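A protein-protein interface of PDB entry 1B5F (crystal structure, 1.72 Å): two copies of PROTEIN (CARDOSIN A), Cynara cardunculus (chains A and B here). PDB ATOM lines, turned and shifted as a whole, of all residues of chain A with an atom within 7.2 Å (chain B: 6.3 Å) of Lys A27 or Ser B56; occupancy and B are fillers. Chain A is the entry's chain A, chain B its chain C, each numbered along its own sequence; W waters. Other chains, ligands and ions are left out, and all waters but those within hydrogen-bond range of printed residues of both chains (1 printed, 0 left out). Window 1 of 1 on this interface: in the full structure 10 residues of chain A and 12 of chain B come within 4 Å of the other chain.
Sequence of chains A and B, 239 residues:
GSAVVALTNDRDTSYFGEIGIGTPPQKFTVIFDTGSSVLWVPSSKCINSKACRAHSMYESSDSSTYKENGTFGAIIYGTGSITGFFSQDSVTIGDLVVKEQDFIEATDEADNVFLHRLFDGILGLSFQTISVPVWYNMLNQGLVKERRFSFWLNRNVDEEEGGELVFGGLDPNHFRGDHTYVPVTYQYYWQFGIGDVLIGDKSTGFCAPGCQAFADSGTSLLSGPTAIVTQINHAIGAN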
ATOM      1  N   GLU A  18      14.168 -15.178  21.696  1.00  0.00           N
ATOM      2  CA  GLU A  18      15.396 -14.944  22.451  1.00  0.00           C
ATOM      3  C   GLU A  18      16.488 -15.884  21.991  1.00  0.00           C
ATOM      4  O   GLU A  18      16.279 -17.037  21.620  1.00  0.00           O
ATOM      5  CB  GLU A  18      15.117 -15.075  23.944  1.00  0.00           C
ATOM      6  CG  GLU A  18      16.287 -15.040  24.908  1.00  0.00           C
ATOM      7  CD  GLU A  18      16.027 -15.793  26.206  1.00  0.00           C
ATOM      8  OE1 GLU A  18      15.044 -15.463  26.911  1.00  0.00           O
ATOM      9  OE2 GLU A  18      16.779 -16.727  26.557  1.00  0.00           O
ATOM     10  N   ILE A  19      17.696 -15.321  22.031  1.00  0.00           N
ATOM     11  CA  ILE A  19      18.895 -16.127  21.938  1.00  0.00           C
ATOM     12  C   ILE A  19      19.881 -15.631  23.001  1.00  0.00           C
ATOM     13  O   ILE A  19      19.663 -14.533  23.516  1.00  0.00           O
ATOM     14  CB  ILE A  19      19.615 -16.017  20.586  1.00  0.00           C
ATOM     15  CG1 ILE A  19      20.116 -14.586  20.342  1.00  0.00           C
ATOM     16  CG2 ILE A  19      18.751 -16.532  19.463  1.00  0.00           C
ATOM     17  CD1 ILE A  19      20.995 -14.444  19.120  1.00  0.00           C
ATOM     18  N   GLY A  20      20.898 -16.448  23.236  1.00  0.00           N
ATOM     19  CA  GLY A  20      22.021 -16.077  24.080  1.00  0.00           C
ATOM     20  C   GLY A  20      23.297 -16.150  23.248  1.00  0.00           C
ATOM     21  O   GLY A  20      23.428 -17.031  22.402  1.00  0.00           O
ATOM     22  N   ILE A  21      24.191 -15.201  23.490  1.00  0.00           N
ATOM     23  CA  ILE A  21      25.502 -15.219  22.852  1.00  0.00           C
ATOM     24  C   ILE A  21      26.564 -15.079  23.936  1.00  0.00           C
ATOM     25  O   ILE A  21      26.484 -14.159  24.748  1.00  0.00           O
ATOM     26  CB  ILE A  21      25.666 -14.128  21.781  1.00  0.00           C
ATOM     27  CG1 ILE A  21      24.571 -14.173  20.709  1.00  0.00           C
ATOM     28  CG2 ILE A  21      27.029 -14.228  21.132  1.00  0.00           C
ATOM     29  CD1 ILE A  21      24.651 -13.035  19.719  1.00  0.00           C
ATOM     30  N   PRO A  24      29.014 -16.598  30.188  1.00  0.00           N
ATOM     31  CA  PRO A  24      27.616 -17.056  30.217  1.00  0.00           C
ATOM     32  C   PRO A  24      26.811 -16.294  29.162  1.00  0.00           C
ATOM     33  O   PRO A  24      27.297 -15.290  28.640  1.00  0.00           O
ATOM     34  CB  PRO A  24      27.110 -16.672  31.595  1.00  0.00           C
ATOM     35  CG  PRO A  24      27.958 -15.498  31.950  1.00  0.00           C
ATOM     36  CD  PRO A  24      29.309 -15.762  31.359  1.00  0.00           C
ATOM     37  N   PRO A  25      25.638 -16.780  28.822  1.00  0.00           N
ATOM     38  CA  PRO A  25      24.936 -16.229  27.650  1.00  0.00           C
ATOM     39  C   PRO A  25      24.421 -14.821  27.875  1.00  0.00           C
ATOM     40  O   PRO A  25      23.669 -14.522  28.793  1.00  0.00           O
ATOM     41  CB  PRO A  25      23.792 -17.225  27.459  1.00  0.00           C
ATOM     42  CG  PRO A  25      24.071 -18.401  28.322  1.00  0.00           C
ATOM     43  CD  PRO A  25      24.892 -17.875  29.471  1.00  0.00           C
ATOM     44  N   GLN A  26      24.816 -13.900  26.993  1.00  0.00           N
ATOM     45  CA  GLN A  26      24.251 -12.560  27.000  1.00  0.00           C
ATOM     46  C   GLN A  26      22.949 -12.600  26.202  1.00  0.00           C
ATOM     47  O   GLN A  26      22.941 -13.223  25.136  1.00  0.00           O
ATOM     48  CB  GLN A  26      25.239 -11.542  26.428  1.00  0.00           C
ATOM     49  CG  GLN A  26      26.530 -11.477  27.243  1.00  0.00           C
ATOM     50  CD  GLN A  26      27.637 -10.701  26.560  1.00  0.00           C
ATOM     51  OE1 GLN A  26      27.390  -9.627  26.028  1.00  0.00           O
ATOM     52  NE2 GLN A  26      28.858 -11.221  26.575  1.00  0.00           N
ATOM     53  N   LYS A  27      21.879 -11.983  26.702  1.00  0.00           N
ATOM     54  CA  LYS A  27      20.595 -12.167  26.036  1.00  0.00           C
ATOM     55  C   LYS A  27      20.326 -11.147  24.944  1.00  0.00           C
ATOM     56  O   LYS A  27      20.626  -9.976  25.119  1.00  0.00           O
ATOM     57  CB  LYS A  27      19.454 -12.077  27.055  1.00  0.00           C
ATOM     58  CG  LYS A  27      18.465 -13.230  27.011  1.00  0.00           C
ATOM     59  CD  LYS A  27      17.220 -12.919  27.823  1.00  0.00           C
ATOM     60  CE  LYS A  27      17.282 -13.501  29.228  1.00  0.00           C
ATOM     61  NZ  LYS A  27      16.229 -12.909  30.117  1.00  0.00           N
ATOM     62  N   PHE A  28      19.736 -11.625  23.854  1.00  0.00           N
ATOM     63  CA  PHE A  28      19.269 -10.804  22.767  1.00  0.00           C
ATOM     64  C   PHE A  28      17.908 -11.268  22.246  1.00  0.00           C
ATOM     65  O   PHE A  28      17.597 -12.450  22.247  1.00  0.00           O
ATOM     66  CB  PHE A  28      20.226 -10.817  21.560  1.00  0.00           C
ATOM     67  CG  PHE A  28      21.608 -10.327  22.011  1.00  0.00           C
ATOM     68  CD1 PHE A  28      22.522 -11.243  22.484  1.00  0.00           C
ATOM     69  CD2 PHE A  28      21.934  -8.985  21.949  1.00  0.00           C
ATOM     70  CE1 PHE A  28      23.758 -10.798  22.907  1.00  0.00           C
ATOM     71  CE2 PHE A  28      23.169  -8.535  22.379  1.00  0.00           C
ATOM     72  CZ  PHE A  28      24.081  -9.454  22.856  1.00  0.00           C
ATOM     73  N   THR A  29      17.168 -10.269  21.825  1.00  0.00           N
ATOM     74  CA  THR A  29      15.907 -10.431  21.120  1.00  0.00           C
ATOM     75  C   THR A  29      16.189 -10.278  19.631  1.00  0.00           C
ATOM     76  O   THR A  29      16.714  -9.263  19.182  1.00  0.00           O
ATOM     77  CB  THR A  29      14.885  -9.406  21.632  1.00  0.00           C
ATOM     78  OG1 THR A  29      14.589  -9.716  23.013  1.00  0.00           O
ATOM     79  CG2 THR A  29      13.578  -9.528  20.872  1.00  0.00           C
ATOM     80  N   VAL A  41      24.087  -8.647  16.057  1.00  0.00           N
ATOM     81  CA  VAL A  41      23.597  -7.977  17.237  1.00  0.00           C
ATOM     82  C   VAL A  41      24.406  -6.692  17.459  1.00  0.00           C
ATOM     83  O   VAL A  41      25.507  -6.560  16.930  1.00  0.00           O
ATOM     84  CB  VAL A  41      23.687  -8.853  18.499  1.00  0.00           C
ATOM     85  CG1 VAL A  41      22.711 -10.026  18.443  1.00  0.00           C
ATOM     86  CG2 VAL A  41      25.117  -9.342  18.672  1.00  0.00           C
ATOM     87  N   SER A  56      20.023  -4.076  23.528  1.00  0.00           N
ATOM     88  CA  SER A  56      21.010  -4.927  24.189  1.00  0.00           C
ATOM     89  C   SER A  56      22.253  -5.094  23.329  1.00  0.00           C
ATOM     90  O   SER A  56      22.171  -5.271  22.107  1.00  0.00           O
ATOM     91  CB  SER A  56      20.420  -6.302  24.520  1.00  0.00           C
ATOM     92  OG  SER A  56      19.209  -6.158  25.238  1.00  0.00           O
ATOM     93  N   MET A  57      23.400  -5.041  23.992  1.00  0.00           N
ATOM     94  CA  MET A  57      24.679  -5.050  23.295  1.00  0.00           C
ATOM     95  C   MET A  57      25.524  -6.249  23.688  1.00  0.00           C
ATOM     96  O   MET A  57      25.395  -6.841  24.760  1.00  0.00           O
ATOM     97  CB  MET A  57      25.419  -3.736  23.560  1.00  0.00           C
ATOM     98  CG  MET A  57      24.650  -2.532  23.023  1.00  0.00           C
ATOM     99  SD  MET A  57      25.079  -0.996  23.863  1.00  0.00           S
ATOM    100  CE  MET A  57      23.738  -0.892  25.055  1.00  0.00           C
ATOM    101  N   TYR A  58      26.422  -6.641  22.790  1.00  0.00           N
ATOM    102  CA  TYR A  58      27.320  -7.739  23.089  1.00  0.00           C
ATOM    103  C   TYR A  58      28.688  -7.250  23.562  1.00  0.00           C
ATOM    104  O   TYR A  58      29.301  -6.438  22.878  1.00  0.00           O
ATOM    105  CB  TYR A  58      27.530  -8.577  21.844  1.00  0.00           C
ATOM    106  CG  TYR A  58      28.572  -9.651  21.898  1.00  0.00           C
ATOM    107  CD1 TYR A  58      28.403 -10.779  22.682  1.00  0.00           C
ATOM    108  CD2 TYR A  58      29.734  -9.552  21.145  1.00  0.00           C
ATOM    109  CE1 TYR A  58      29.366 -11.764  22.720  1.00  0.00           C
ATOM    110  CE2 TYR A  58      30.698 -10.530  21.179  1.00  0.00           C
ATOM    111  CZ  TYR A  58      30.515 -11.638  21.970  1.00  0.00           C
ATOM    112  OH  TYR A  58      31.473 -12.621  22.002  1.00  0.00           O
ATOM    113  N   ASP A 120      16.636  -6.533  19.004  1.00  0.00           N
ATOM    114  CA  ASP A 120      18.018  -6.116  19.068  1.00  0.00           C
ATOM    115  C   ASP A 120      18.789  -6.373  17.781  1.00  0.00           C
ATOM    116  O   ASP A 120      19.575  -5.524  17.368  1.00  0.00           O
ATOM    117  CB  ASP A 120      18.764  -6.846  20.197  1.00  0.00           C
ATOM    118  CG  ASP A 120      18.107  -6.514  21.533  1.00  0.00           C
ATOM    119  OD1 ASP A 120      17.958  -5.294  21.752  1.00  0.00           O
ATOM    120  OD2 ASP A 120      17.772  -7.459  22.264  1.00  0.00           O
ATOM    121  N   GLU B  18      15.482 -20.029  34.060  1.00  0.00           N
ATOM    122  CA  GLU B  18      14.347 -19.361  33.421  1.00  0.00           C
ATOM    123  C   GLU B  18      13.034 -19.604  34.130  1.00  0.00           C
ATOM    124  O   GLU B  18      12.763 -20.681  34.646  1.00  0.00           O
ATOM    125  CB  GLU B  18      14.295 -19.833  31.963  1.00  0.00           C
ATOM    126  CG  GLU B  18      15.557 -19.388  31.230  1.00  0.00           C
ATOM    127  CD  GLU B  18      15.995 -17.989  31.611  1.00  0.00           C
ATOM    128  OE1 GLU B  18      15.129 -17.144  31.908  1.00  0.00           O
ATOM    129  OE2 GLU B  18      17.211 -17.707  31.608  1.00  0.00           O
ATOM    130  N   LYS B  27       9.185 -14.499  29.411  1.00  0.00           N
ATOM    131  CA  LYS B  27      10.327 -15.187  30.027  1.00  0.00           C
ATOM    132  C   LYS B  27      11.287 -14.249  30.754  1.00  0.00           C
ATOM    133  O   LYS B  27      11.634 -13.108  30.460  1.00  0.00           O
ATOM    134  CB  LYS B  27      11.090 -15.939  28.923  1.00  0.00           C
ATOM    135  CG  LYS B  27      10.333 -17.079  28.271  1.00  0.00           C
ATOM    136  CD  LYS B  27      10.822 -17.427  26.875  1.00  0.00           C
ATOM    137  CE  LYS B  27      10.110 -18.644  26.292  1.00  0.00           C
ATOM    138  NZ  LYS B  27       8.698 -18.754  26.779  1.00  0.00           N
ATOM    139  N   PHE B  28      11.764 -14.777  31.889  1.00  0.00           N
ATOM    140  CA  PHE B  28      12.695 -14.105  32.757  1.00  0.00           C
ATOM    141  C   PHE B  28      13.760 -15.100  33.236  1.00  0.00           C
ATOM    142  O   PHE B  28      13.473 -16.281  33.401  1.00  0.00           O
ATOM    143  CB  PHE B  28      12.031 -13.494  33.997  1.00  0.00           C
ATOM    144  CG  PHE B  28      10.948 -12.508  33.572  1.00  0.00           C
ATOM    145  CD1 PHE B  28       9.674 -12.964  33.318  1.00  0.00           C
ATOM    146  CD2 PHE B  28      11.270 -11.168  33.430  1.00  0.00           C
ATOM    147  CE1 PHE B  28       8.706 -12.049  32.909  1.00  0.00           C
ATOM    148  CE2 PHE B  28      10.306 -10.250  33.032  1.00  0.00           C
ATOM    149  CZ  PHE B  28       9.039 -10.720  32.774  1.00  0.00           C
ATOM    150  N   THR B  29      14.926 -14.521  33.413  1.00  0.00           N
ATOM    151  CA  THR B  29      16.078 -15.122  34.045  1.00  0.00           C
ATOM    152  C   THR B  29      16.156 -14.617  35.477  1.00  0.00           C
ATOM    153  O   THR B  29      16.255 -13.417  35.749  1.00  0.00           O
ATOM    154  CB  THR B  29      17.339 -14.742  33.255  1.00  0.00           C
ATOM    155  OG1 THR B  29      17.255 -15.452  31.996  1.00  0.00           O
ATOM    156  CG2 THR B  29      18.584 -15.224  33.947  1.00  0.00           C
ATOM    157  N   VAL B  41      10.599  -9.054  39.373  1.00  0.00           N
ATOM    158  CA  VAL B  41      11.208  -8.882  38.064  1.00  0.00           C
ATOM    159  C   VAL B  41      11.018  -7.427  37.638  1.00  0.00           C
ATOM    160  O   VAL B  41      10.185  -6.717  38.232  1.00  0.00           O
ATOM    161  CB  VAL B  41      10.575  -9.809  37.033  1.00  0.00           C
ATOM    162  CG1 VAL B  41      10.754 -11.287  37.350  1.00  0.00           C
ATOM    163  CG2 VAL B  41       9.075  -9.506  36.939  1.00  0.00           C
ATOM    164  N   PRO B  42      11.746  -6.964  36.635  1.00  0.00           N
ATOM    165  CA  PRO B  42      11.575  -5.578  36.163  1.00  0.00           C
ATOM    166  C   PRO B  42      10.221  -5.375  35.492  1.00  0.00           C
ATOM    167  O   PRO B  42       9.676  -6.245  34.798  1.00  0.00           O
ATOM    168  CB  PRO B  42      12.723  -5.413  35.173  1.00  0.00           C
ATOM    169  CG  PRO B  42      13.702  -6.481  35.582  1.00  0.00           C
ATOM    170  CD  PRO B  42      12.791  -7.663  35.863  1.00  0.00           C
ATOM    171  N   SER B  43       9.669  -4.182  35.736  1.00  0.00           N
ATOM    172  CA  SER B  43       8.371  -3.802  35.219  1.00  0.00           C
ATOM    173  C   SER B  43       8.439  -3.134  33.856  1.00  0.00           C
ATOM    174  O   SER B  43       9.375  -2.393  33.601  1.00  0.00           O
ATOM    175  CB  SER B  43       7.664  -2.757  36.115  1.00  0.00           C
ATOM    176  OG  SER B  43       6.331  -2.651  35.615  1.00  0.00           O
ATOM    177  N   CYS B  52      16.507  -1.703  34.739  1.00  0.00           N
ATOM    178  CA  CYS B  52      15.256  -2.271  34.249  1.00  0.00           C
ATOM    179  C   CYS B  52      15.308  -2.374  32.720  1.00  0.00           C
ATOM    180  O   CYS B  52      14.986  -3.409  32.143  1.00  0.00           O
ATOM    181  CB  CYS B  52      14.015  -1.476  34.626  1.00  0.00           C
ATOM    182  SG  CYS B  52      13.603  -1.253  36.359  1.00  0.00           S
ATOM    183  N   ARG B  53      15.710  -1.299  32.043  1.00  0.00           N
ATOM    184  CA  ARG B  53      15.652  -1.313  30.579  1.00  0.00           C
ATOM    185  C   ARG B  53      16.717  -2.210  29.978  1.00  0.00           C
ATOM    186  O   ARG B  53      16.604  -2.639  28.832  1.00  0.00           O
ATOM    187  CB  ARG B  53      15.770   0.109  30.025  1.00  0.00           C
ATOM    188  CG  ARG B  53      14.662   0.459  29.042  1.00  0.00           C
ATOM    189  CD  ARG B  53      15.053   0.031  27.635  1.00  0.00           C
ATOM    190  NE  ARG B  53      15.365   1.175  26.782  1.00  0.00           N
ATOM    191  CZ  ARG B  53      14.463   1.931  26.165  1.00  0.00           C
ATOM    192  NH1 ARG B  53      13.165   1.675  26.303  1.00  0.00           N
ATOM    193  NH2 ARG B  53      14.849   2.951  25.405  1.00  0.00           N
ATOM    194  N   ALA B  54      17.767  -2.528  30.732  1.00  0.00           N
ATOM    195  CA  ALA B  54      18.710  -3.519  30.195  1.00  0.00           C
ATOM    196  C   ALA B  54      18.159  -4.934  30.319  1.00  0.00           C
ATOM    197  O   ALA B  54      18.732  -5.913  29.848  1.00  0.00           O
ATOM    198  CB  ALA B  54      20.062  -3.440  30.886  1.00  0.00           C
ATOM    199  N   HIS B  55      17.014  -5.088  30.978  1.00  0.00           N
ATOM    200  CA  HIS B  55      16.579  -6.454  31.254  1.00  0.00           C
ATOM    201  C   HIS B  55      15.203  -6.759  30.707  1.00  0.00           C
ATOM    202  O   HIS B  55      14.448  -5.885  30.286  1.00  0.00           O
ATOM    203  CB  HIS B  55      16.643  -6.633  32.789  1.00  0.00           C
ATOM    204  CG  HIS B  55      18.056  -6.818  33.231  1.00  0.00           C
ATOM    205  ND1 HIS B  55      18.811  -5.818  33.792  1.00  0.00           N
ATOM    206  CD2 HIS B  55      18.856  -7.909  33.194  1.00  0.00           C
ATOM    207  CE1 HIS B  55      20.015  -6.277  34.080  1.00  0.00           C
ATOM    208  NE2 HIS B  55      20.073  -7.550  33.726  1.00  0.00           N
ATOM    209  N   SER B  56      14.832  -8.046  30.718  1.00  0.00           N
ATOM    210  CA  SER B  56      13.457  -8.373  30.370  1.00  0.00           C
ATOM    211  C   SER B  56      12.509  -7.693  31.359  1.00  0.00           C
ATOM    212  O   SER B  56      12.810  -7.688  32.556  1.00  0.00           O
ATOM    213  CB  SER B  56      13.303  -9.898  30.307  1.00  0.00           C
ATOM    214  OG  SER B  56      14.221 -10.410  29.332  1.00  0.00           O
ATOM    215  N   MET B  57      11.419  -7.127  30.868  1.00  0.00           N
ATOM    216  CA  MET B  57      10.373  -6.419  31.588  1.00  0.00           C
ATOM    217  C   MET B  57       9.010  -7.093  31.507  1.00  0.00           C
ATOM    218  O   MET B  57       8.609  -7.674  30.492  1.00  0.00           O
ATOM    219  CB  MET B  57      10.231  -4.989  31.048  1.00  0.00           C
ATOM    220  CG  MET B  57      11.417  -4.137  31.497  1.00  0.00           C
ATOM    221  SD  MET B  57      11.477  -2.552  30.611  1.00  0.00           S
ATOM    222  CE  MET B  57      12.729  -3.002  29.390  1.00  0.00           C
ATOM    223  N   TYR B  58       8.292  -6.994  32.629  1.00  0.00           N
ATOM    224  CA  TYR B  58       6.976  -7.605  32.682  1.00  0.00           C
ATOM    225  C   TYR B  58       5.904  -6.612  32.203  1.00  0.00           C
ATOM    226  O   TYR B  58       5.922  -5.477  32.684  1.00  0.00           O
ATOM    227  CB  TYR B  58       6.607  -8.016  34.105  1.00  0.00           C
ATOM    228  CG  TYR B  58       5.194  -8.555  34.222  1.00  0.00           C
ATOM    229  CD1 TYR B  58       4.824  -9.769  33.678  1.00  0.00           C
ATOM    230  CD2 TYR B  58       4.225  -7.814  34.894  1.00  0.00           C
ATOM    231  CE1 TYR B  58       3.538 -10.278  33.774  1.00  0.00           C
ATOM    232  CE2 TYR B  58       2.939  -8.305  34.999  1.00  0.00           C
ATOM    233  CZ  TYR B  58       2.605  -9.513  34.446  1.00  0.00           C
ATOM    234  OH  TYR B  58       1.322  -9.992  34.565  1.00  0.00           O
ATOM    235  N   LEU B 118      23.463 -10.522  34.768  1.00  0.00           N
ATOM    236  CA  LEU B 118      22.726 -11.145  33.669  1.00  0.00           C
ATOM    237  C   LEU B 118      21.308 -11.556  34.030  1.00  0.00           C
ATOM    238  O   LEU B 118      20.505 -11.701  33.108  1.00  0.00           O
ATOM    239  CB  LEU B 118      23.475 -12.371  33.133  1.00  0.00           C
ATOM    240  CG  LEU B 118      24.711 -11.991  32.300  1.00  0.00           C
ATOM    241  CD1 LEU B 118      25.699 -13.134  32.332  1.00  0.00           C
ATOM    242  CD2 LEU B 118      24.293 -11.601  30.886  1.00  0.00           C
ATOM    243  N   ASP B 120      17.451 -11.146  35.335  1.00  0.00           N
ATOM    244  CA  ASP B 120      16.387 -10.159  35.308  1.00  0.00           C
ATOM    245  C   ASP B 120      15.794  -9.878  36.684  1.00  0.00           C
ATOM    246  O   ASP B 120      15.522  -8.738  37.082  1.00  0.00           O
ATOM    247  CB  ASP B 120      15.262 -10.646  34.395  1.00  0.00           C
ATOM    248  CG  ASP B 120      15.760 -10.864  32.971  1.00  0.00           C
ATOM    249  OD1 ASP B 120      16.484  -9.971  32.482  1.00  0.00           O
ATOM    250  OD2 ASP B 120      15.415 -11.911  32.377  1.00  0.00           O
HETATM  251  O   HOH W   1      14.977 -15.217  29.411  1.00  0.00           O
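The side-chain carboxylate (OE1) of Glu B18 sits at hydrogen-bond distance from the side-chain hydroxyl (OG1) of Thr B29, at 2.7 Å.
The backbone NH (N) of Asp B120 is in hydrogen-bond range of the backbone carbonyl oxygen (O) of Thr B29 (2.6 Å).
N of Ser B56 sits at hydrogen-bond distance from OD1 of Asp B120.
OG1 of Thr B29 sits at hydrogen-bond distance from NZ of Lys A27, at 3.3 Å.
The side-chain amino group (NZ) of Lys A27 lies within hydrogen-bond range of the side-chain hydroxyl (OG) of Ser B56, at 3.3 Å.
The side-chain carboxylate of Asp B120 is in salt-bridge range of the side-chain amino group of Lys A27, 2.6 Å away.
Lys A27 touches Thr B29, but with the chains exchanged Thr A29 does not touch Lys B27 (8.7 Å).
Lys A27 touches Ser B56, but with the chains exchanged Ser A56 does not touch Lys B27 (11.5 Å).
Lys A27 touches Asp B120, but with the chains exchanged Asp A120 does not touch Lys B27 (11.7 Å).
Of the 5 pairs that touch across the chains among the printed residues, none has its exchanged pair printed and touching as well.
Of the 15 printed residues of chain A, 3 touch a printed residue of chain B.
Printed residues of chain B that touch a printed residue of chain A: Thr B29, Ser B56, Leu B118 and Asp B120.
Along chain B the printed residues that touch a printed residue of chain A span positions 29 to 120.
Among the printed residues, 5 pairs touch across the chains.
Among the printed residues, pairs that only touch across the chains: Pro A24 with Leu B118 (3.3 Å) and Pro A25 with Leu B118 (3.6 Å).
Of chain B, only Thr B29, Ser B56 and Asp B120 come within 4 Å of Lys A27.
Ser B56 touches just one residue of chain A: Lys A27.
Of the printed residues of chain B, Pro A25 touches Leu B118 (3.6 Å).
Of the printed residues of chain B, Pro A24 touches Leu B118.
Of the printed residues of chain A, Asp B120 touches Lys A27 (2.6 Å).
Ser B43 touches none of the printed residues of chain A.
The nearest residue of chain B that does not touch Lys A27 is Phe B28 (4.5 Å).
The nearest residue of chain A that does not touch Ser B56 is Glu A18 (5.7 Å).
Water W1 lies within hydrogen-bond range of OE1 of Glu A18, NZ of Lys A27, OE1 of Glu B18 and OG1 of Thr B29.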
